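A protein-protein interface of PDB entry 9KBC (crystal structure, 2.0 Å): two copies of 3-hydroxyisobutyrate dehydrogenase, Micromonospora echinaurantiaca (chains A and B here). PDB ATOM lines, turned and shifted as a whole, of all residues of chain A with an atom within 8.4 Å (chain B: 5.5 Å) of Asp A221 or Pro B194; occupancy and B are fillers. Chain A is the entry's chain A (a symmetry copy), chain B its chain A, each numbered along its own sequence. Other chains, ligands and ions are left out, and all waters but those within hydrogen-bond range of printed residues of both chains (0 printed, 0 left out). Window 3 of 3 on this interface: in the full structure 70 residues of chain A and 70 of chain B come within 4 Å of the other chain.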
ATOM      1  N   HIS A 166     -30.660 -29.595 -13.471  1.00  0.00           N
ATOM      2  CA  HIS A 166     -31.412 -28.497 -12.870  1.00  0.00           C
ATOM      3  C   HIS A 166     -31.676 -28.748 -11.391  1.00  0.00           C
ATOM      4  O   HIS A 166     -31.647 -27.812 -10.584  1.00  0.00           O
ATOM      5  CB  HIS A 166     -32.722 -28.280 -13.628  1.00  0.00           C
ATOM      6  CG  HIS A 166     -32.536 -27.692 -14.993  1.00  0.00           C
ATOM      7  ND1 HIS A 166     -31.994 -28.404 -16.042  1.00  0.00           N
ATOM      8  CD2 HIS A 166     -32.808 -26.457 -15.478  1.00  0.00           C
ATOM      9  CE1 HIS A 166     -31.946 -27.634 -17.115  1.00  0.00           C
ATOM     10  NE2 HIS A 166     -32.432 -26.447 -16.799  1.00  0.00           N
ATOM     11  N   PRO A 214     -32.549 -11.531 -13.119  1.00  0.00           N
ATOM     12  CA  PRO A 214     -32.669 -11.396 -14.582  1.00  0.00           C
ATOM     13  C   PRO A 214     -31.553 -10.580 -15.214  1.00  0.00           C
ATOM     14  O   PRO A 214     -31.080 -10.932 -16.303  1.00  0.00           O
ATOM     15  CB  PRO A 214     -34.039 -10.725 -14.747  1.00  0.00           C
ATOM     16  CG  PRO A 214     -34.812 -11.237 -13.588  1.00  0.00           C
ATOM     17  CD  PRO A 214     -33.824 -11.196 -12.454  1.00  0.00           C
ATOM     18  N   ALA A 215     -31.110  -9.504 -14.560  1.00  0.00           N
ATOM     19  CA  ALA A 215     -30.014  -8.711 -15.108  1.00  0.00           C
ATOM     20  C   ALA A 215     -28.700  -9.485 -15.073  1.00  0.00           C
ATOM     21  O   ALA A 215     -27.894  -9.390 -16.006  1.00  0.00           O
ATOM     22  CB  ALA A 215     -29.883  -7.391 -14.348  1.00  0.00           C
ATOM     23  N   LEU A 216     -28.464 -10.250 -14.004  1.00  0.00           N
ATOM     24  CA  LEU A 216     -27.281 -11.103 -13.960  1.00  0.00           C
ATOM     25  C   LEU A 216     -27.301 -12.125 -15.089  1.00  0.00           C
ATOM     26  O   LEU A 216     -26.280 -12.352 -15.750  1.00  0.00           O
ATOM     27  CB  LEU A 216     -27.189 -11.815 -12.610  1.00  0.00           C
ATOM     28  CG  LEU A 216     -26.835 -10.991 -11.375  1.00  0.00           C
ATOM     29  CD1 LEU A 216     -26.938 -11.847 -10.122  1.00  0.00           C
ATOM     30  CD2 LEU A 216     -25.440 -10.402 -11.512  1.00  0.00           C
ATOM     31  N   ALA A 217     -28.455 -12.751 -15.324  1.00  0.00           N
ATOM     32  CA  ALA A 217     -28.546 -13.779 -16.354  1.00  0.00           C
ATOM     33  C   ALA A 217     -28.260 -13.209 -17.737  1.00  0.00           C
ATOM     34  O   ALA A 217     -27.589 -13.851 -18.554  1.00  0.00           O
ATOM     35  CB  ALA A 217     -29.924 -14.436 -16.317  1.00  0.00           C
ATOM     36  N   ARG A 218     -28.756 -11.998 -18.018  1.00  0.00           N
ATOM     37  CA  ARG A 218     -28.517 -11.382 -19.321  1.00  0.00           C
ATOM     38  C   ARG A 218     -27.035 -11.108 -19.538  1.00  0.00           C
ATOM     39  O   ARG A 218     -26.498 -11.379 -20.619  1.00  0.00           O
ATOM     40  CB  ARG A 218     -29.324 -10.090 -19.448  1.00  0.00           C
ATOM     41  CG  ARG A 218     -30.809 -10.310 -19.681  1.00  0.00           C
ATOM     42  CD  ARG A 218     -31.491  -9.027 -20.131  1.00  0.00           C
ATOM     43  NE  ARG A 218     -31.737  -8.124 -19.013  1.00  0.00           N
ATOM     44  CZ  ARG A 218     -32.740  -8.247 -18.156  1.00  0.00           C
ATOM     45  NH1 ARG A 218     -33.625  -9.225 -18.264  1.00  0.00           N
ATOM     46  NH2 ARG A 218     -32.859  -7.367 -17.166  1.00  0.00           N
ATOM     47  N   GLY A 219     -26.356 -10.573 -18.523  1.00  0.00           N
ATOM     48  CA  GLY A 219     -24.928 -10.334 -18.642  1.00  0.00           C
ATOM     49  C   GLY A 219     -24.127 -11.605 -18.843  1.00  0.00           C
ATOM     50  O   GLY A 219     -23.111 -11.601 -19.545  1.00  0.00           O
ATOM     51  N   VAL A 220     -24.570 -12.707 -18.236  1.00  0.00           N
ATOM     52  CA  VAL A 220     -23.888 -13.983 -18.422  1.00  0.00           C
ATOM     53  C   VAL A 220     -24.077 -14.489 -19.848  1.00  0.00           C
ATOM     54  O   VAL A 220     -23.123 -14.939 -20.495  1.00  0.00           O
ATOM     55  CB  VAL A 220     -24.389 -15.007 -17.387  1.00  0.00           C
ATOM     56  CG1 VAL A 220     -23.909 -16.402 -17.744  1.00  0.00           C
ATOM     57  CG2 VAL A 220     -23.929 -14.615 -15.987  1.00  0.00           C
ATOM     58  N   ASP A 221     -25.304 -14.411 -20.364  1.00  0.00           N
ATOM     59  CA  ASP A 221     -25.583 -14.964 -21.685  1.00  0.00           C
ATOM     60  C   ASP A 221     -25.013 -14.085 -22.792  1.00  0.00           C
ATOM     61  O   ASP A 221     -24.540 -14.595 -23.816  1.00  0.00           O
ATOM     62  CB  ASP A 221     -27.090 -15.147 -21.866  1.00  0.00           C
ATOM     63  CG  ASP A 221     -27.628 -16.348 -21.106  1.00  0.00           C
ATOM     64  OD1 ASP A 221     -26.818 -17.181 -20.650  1.00  0.00           O
ATOM     65  OD2 ASP A 221     -28.865 -16.454 -20.962  1.00  0.00           O
ATOM     66  N   SER A 222     -25.044 -12.765 -22.610  1.00  0.00           N
ATOM     67  CA  SER A 222     -24.566 -11.854 -23.641  1.00  0.00           C
ATOM     68  C   SER A 222     -23.065 -11.614 -23.578  1.00  0.00           C
ATOM     69  O   SER A 222     -22.476 -11.197 -24.582  1.00  0.00           O
ATOM     70  CB  SER A 222     -25.299 -10.511 -23.542  1.00  0.00           C
ATOM     71  OG  SER A 222     -24.958  -9.825 -22.350  1.00  0.00           O
ATOM     72  N   GLY A 223     -22.432 -11.883 -22.439  1.00  0.00           N
ATOM     73  CA  GLY A 223     -21.038 -11.554 -22.260  1.00  0.00           C
ATOM     74  C   GLY A 223     -20.769 -10.116 -21.873  1.00  0.00           C
ATOM     75  O   GLY A 223     -19.608  -9.766 -21.629  1.00  0.00           O
ATOM     76  N   ASP A 224     -21.799  -9.274 -21.815  1.00  0.00           N
ATOM     77  CA  ASP A 224     -21.663  -7.889 -21.365  1.00  0.00           C
ATOM     78  C   ASP A 224     -21.885  -7.872 -19.860  1.00  0.00           C
ATOM     79  O   ASP A 224     -23.022  -7.907 -19.387  1.00  0.00           O
ATOM     80  CB  ASP A 224     -22.653  -6.986 -22.089  1.00  0.00           C
ATOM     81  CG  ASP A 224     -22.667  -5.561 -21.550  1.00  0.00           C
ATOM     82  OD1 ASP A 224     -21.717  -5.166 -20.843  1.00  0.00           O
ATOM     83  OD2 ASP A 224     -23.635  -4.830 -21.852  1.00  0.00           O
ATOM     84  N   HIS A 225     -20.793  -7.812 -19.106  1.00  0.00           N
ATOM     85  CA  HIS A 225     -20.851  -7.851 -17.648  1.00  0.00           C
ATOM     86  C   HIS A 225     -20.950  -6.448 -17.057  1.00  0.00           C
ATOM     87  O   HIS A 225     -20.195  -6.066 -16.165  1.00  0.00           O
ATOM     88  CB  HIS A 225     -19.638  -8.599 -17.111  1.00  0.00           C
ATOM     89  CG  HIS A 225     -19.488  -9.980 -17.673  1.00  0.00           C
ATOM     90  ND1 HIS A 225     -18.264 -10.598 -17.820  1.00  0.00           N
ATOM     91  CD2 HIS A 225     -20.410 -10.861 -18.127  1.00  0.00           C
ATOM     92  CE1 HIS A 225     -18.439 -11.800 -18.340  1.00  0.00           C
ATOM     93  NE2 HIS A 225     -19.733 -11.984 -18.536  1.00  0.00           N
ATOM     94  N   SER A 277     -22.028 -10.689 -12.827  1.00  0.00           N
ATOM     95  CA  SER A 277     -22.051 -11.673 -13.903  1.00  0.00           C
ATOM     96  C   SER A 277     -20.650 -12.048 -14.372  1.00  0.00           C
ATOM     97  O   SER A 277     -20.478 -13.093 -15.008  1.00  0.00           O
ATOM     98  CB  SER A 277     -22.873 -11.147 -15.080  1.00  0.00           C
ATOM     99  OG  SER A 277     -22.334  -9.928 -15.560  1.00  0.00           O
ATOM    100  N   VAL A 280     -19.047 -15.647 -13.066  1.00  0.00           N
ATOM    101  CA  VAL A 280     -19.434 -16.980 -13.532  1.00  0.00           C
ATOM    102  C   VAL A 280     -18.273 -17.661 -14.250  1.00  0.00           C
ATOM    103  O   VAL A 280     -17.954 -18.826 -13.981  1.00  0.00           O
ATOM    104  CB  VAL A 280     -20.684 -16.895 -14.426  1.00  0.00           C
ATOM    105  CG1 VAL A 280     -20.967 -18.242 -15.070  1.00  0.00           C
ATOM    106  CG2 VAL A 280     -21.883 -16.453 -13.608  1.00  0.00           C
ATOM    107  N   ASP A 281     -17.625 -16.947 -15.178  1.00  0.00           N
ATOM    108  CA  ASP A 281     -16.476 -17.513 -15.884  1.00  0.00           C
ATOM    109  C   ASP A 281     -15.332 -17.839 -14.933  1.00  0.00           C
ATOM    110  O   ASP A 281     -14.554 -18.764 -15.194  1.00  0.00           O
ATOM    111  CB  ASP A 281     -15.983 -16.546 -16.964  1.00  0.00           C
ATOM    112  CG  ASP A 281     -17.006 -16.305 -18.054  1.00  0.00           C
ATOM    113  OD1 ASP A 281     -17.628 -17.284 -18.526  1.00  0.00           O
ATOM    114  OD2 ASP A 281     -17.185 -15.130 -18.445  1.00  0.00           O
ATOM    115  N   ILE B 188     -25.256 -24.663 -15.191  1.00  0.00           N
ATOM    116  CA  ILE B 188     -26.174 -24.573 -16.321  1.00  0.00           C
ATOM    117  C   ILE B 188     -25.416 -24.181 -17.586  1.00  0.00           C
ATOM    118  O   ILE B 188     -25.557 -24.810 -18.643  1.00  0.00           O
ATOM    119  CB  ILE B 188     -27.293 -23.566 -15.991  1.00  0.00           C
ATOM    120  CG1 ILE B 188     -28.310 -24.172 -15.017  1.00  0.00           C
ATOM    121  CG2 ILE B 188     -27.968 -23.065 -17.240  1.00  0.00           C
ATOM    122  CD1 ILE B 188     -28.577 -25.640 -15.227  1.00  0.00           C
ATOM    123  N   ARG B 189     -24.584 -23.140 -17.481  1.00  0.00           N
ATOM    124  CA  ARG B 189     -23.788 -22.672 -18.613  1.00  0.00           C
ATOM    125  C   ARG B 189     -22.899 -23.773 -19.180  1.00  0.00           C
ATOM    126  O   ARG B 189     -22.754 -23.891 -20.403  1.00  0.00           O
ATOM    127  CB  ARG B 189     -22.935 -21.482 -18.178  1.00  0.00           C
ATOM    128  CG  ARG B 189     -22.544 -20.536 -19.287  1.00  0.00           C
ATOM    129  CD  ARG B 189     -21.926 -19.282 -18.693  1.00  0.00           C
ATOM    130  NE  ARG B 189     -20.866 -18.731 -19.528  1.00  0.00           N
ATOM    131  CZ  ARG B 189     -21.078 -18.035 -20.636  1.00  0.00           C
ATOM    132  NH1 ARG B 189     -22.303 -17.812 -21.089  1.00  0.00           N
ATOM    133  NH2 ARG B 189     -20.038 -17.548 -21.306  1.00  0.00           N
ATOM    134  N   GLY B 192     -24.370 -25.822 -21.762  1.00  0.00           N
ATOM    135  CA  GLY B 192     -24.876 -25.119 -22.924  1.00  0.00           C
ATOM    136  C   GLY B 192     -26.290 -24.613 -22.789  1.00  0.00           C
ATOM    137  O   GLY B 192     -26.953 -24.388 -23.808  1.00  0.00           O
ATOM    138  N   VAL B 193     -26.774 -24.428 -21.570  1.00  0.00           N
ATOM    139  CA  VAL B 193     -28.150 -24.011 -21.308  1.00  0.00           C
ATOM    140  C   VAL B 193     -28.137 -22.527 -20.955  1.00  0.00           C
ATOM    141  O   VAL B 193     -27.283 -22.103 -20.163  1.00  0.00           O
ATOM    142  CB  VAL B 193     -28.779 -24.841 -20.172  1.00  0.00           C
ATOM    143  CG1 VAL B 193     -30.165 -24.317 -19.807  1.00  0.00           C
ATOM    144  CG2 VAL B 193     -28.834 -26.311 -20.553  1.00  0.00           C
ATOM    145  N   PRO B 194     -29.034 -21.716 -21.516  1.00  0.00           N
ATOM    146  CA  PRO B 194     -28.997 -20.274 -21.230  1.00  0.00           C
ATOM    147  C   PRO B 194     -29.396 -19.970 -19.795  1.00  0.00           C
ATOM    148  O   PRO B 194     -30.324 -20.569 -19.246  1.00  0.00           O
ATOM    149  CB  PRO B 194     -30.006 -19.679 -22.221  1.00  0.00           C
ATOM    150  CG  PRO B 194     -30.356 -20.782 -23.178  1.00  0.00           C
ATOM    151  CD  PRO B 194     -30.092 -22.071 -22.477  1.00  0.00           C
ATOM    152  N   ALA B 195     -28.688 -19.012 -19.193  1.00  0.00           N
ATOM    153  CA  ALA B 195     -29.044 -18.575 -17.849  1.00  0.00           C
ATOM    154  C   ALA B 195     -30.401 -17.882 -17.824  1.00  0.00           C
ATOM    155  O   ALA B 195     -31.113 -17.959 -16.818  1.00  0.00           O
ATOM    156  CB  ALA B 195     -27.967 -17.643 -17.293  1.00  0.00           C
ATOM    157  N   THR B 196     -30.776 -17.217 -18.921  1.00  0.00           N
ATOM    158  CA  THR B 196     -32.019 -16.449 -18.945  1.00  0.00           C
ATOM    159  C   THR B 196     -33.230 -17.347 -18.718  1.00  0.00           C
ATOM    160  O   THR B 196     -34.113 -17.027 -17.915  1.00  0.00           O
ATOM    161  CB  THR B 196     -32.142 -15.696 -20.273  1.00  0.00           C
ATOM    162  OG1 THR B 196     -31.275 -14.559 -20.256  1.00  0.00           O
ATOM    163  CG2 THR B 196     -33.569 -15.219 -20.486  1.00  0.00           C
ATOM    164  N   GLY B 197     -33.288 -18.482 -19.417  1.00  0.00           N
ATOM    165  CA  GLY B 197     -34.398 -19.399 -19.228  1.00  0.00           C
ATOM    166  C   GLY B 197     -34.382 -20.116 -17.895  1.00  0.00           C
ATOM    167  O   GLY B 197     -35.435 -20.571 -17.432  1.00  0.00           O
ATOM    168  N   PHE B 198     -33.209 -20.226 -17.270  1.00  0.00           N
ATOM    169  CA  PHE B 198     -33.090 -20.889 -15.977  1.00  0.00           C
ATOM    170  C   PHE B 198     -33.556 -19.997 -14.835  1.00  0.00           C
ATOM    171  O   PHE B 198     -34.050 -20.501 -13.821  1.00  0.00           O
ATOM    172  CB  PHE B 198     -31.634 -21.313 -15.757  1.00  0.00           C
ATOM    173  CG  PHE B 198     -31.336 -21.801 -14.364  1.00  0.00           C
ATOM    174  CD1 PHE B 198     -31.744 -23.060 -13.952  1.00  0.00           C
ATOM    175  CD2 PHE B 198     -30.635 -21.006 -13.472  1.00  0.00           C
ATOM    176  CE1 PHE B 198     -31.462 -23.512 -12.672  1.00  0.00           C
ATOM    177  CE2 PHE B 198     -30.354 -21.452 -12.194  1.00  0.00           C
ATOM    178  CZ  PHE B 198     -30.766 -22.705 -11.794  1.00  0.00           C
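The guanidinium group (NH1) of Arg B189 is in hydrogen-bond range of the backbone carbonyl oxygen (O) of Val A220 (3.0 Å). NE of Arg B189 lies within salt-bridge range of OD1 of Asp A281 (3.7 Å). OD1 of Asp A221 is in hydrogen-bond range of N of Ala B195 (3.0 Å). The side-chain carboxylate (OD2) of Asp A221 is in hydrogen-bond range of the backbone NH (N) of Thr B196 (2.9 Å).
Among the printed residues, pairs that only touch across the chains: Asp A221 with Pro B194, Ala A217 with Ala B195, His A166 with Phe B198, Val A280 with Arg B189 and Ala A217 with Thr B196.
No position is printed for both chains.
Of the 9 printed residues of chain B, 5 touch a printed residue of chain A. Printed residues of chain B that touch a printed residue of chain A: Arg B189, Pro B194, Ala B195, Thr B196 and Phe B198. Hydrophobic or aromatic side chains of chain B that line the printed part of chain A: Pro B194, Ala B195 and Phe B198. Of the 16 printed residues of chain A, 6 touch a printed residue of chain B. Hydrophobic or aromatic side chains of chain A that line the printed part of chain B: His A166, Ala A217, Val A220 and Val A280. Among the printed residues, 9 pairs touch across the chains.
Asp A221 touches three residues of chain B. Printed residues of chain A within 4 Å of Pro B194: Asp A221. Printed residues of chain A within 4 Å of Phe B198: His A166 (3.9 Å). Printed residues of chain B within 4 Å of Asp A281: Arg B189. Leu A216 touches none of the printed residues of chain B. The nearest residue of chain A that does not touch Pro B194 is Ala A217 (6.5 Å). The nearest printed residue of chain B that does not touch Asp A281 is Ala B195 (10.4 Å).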
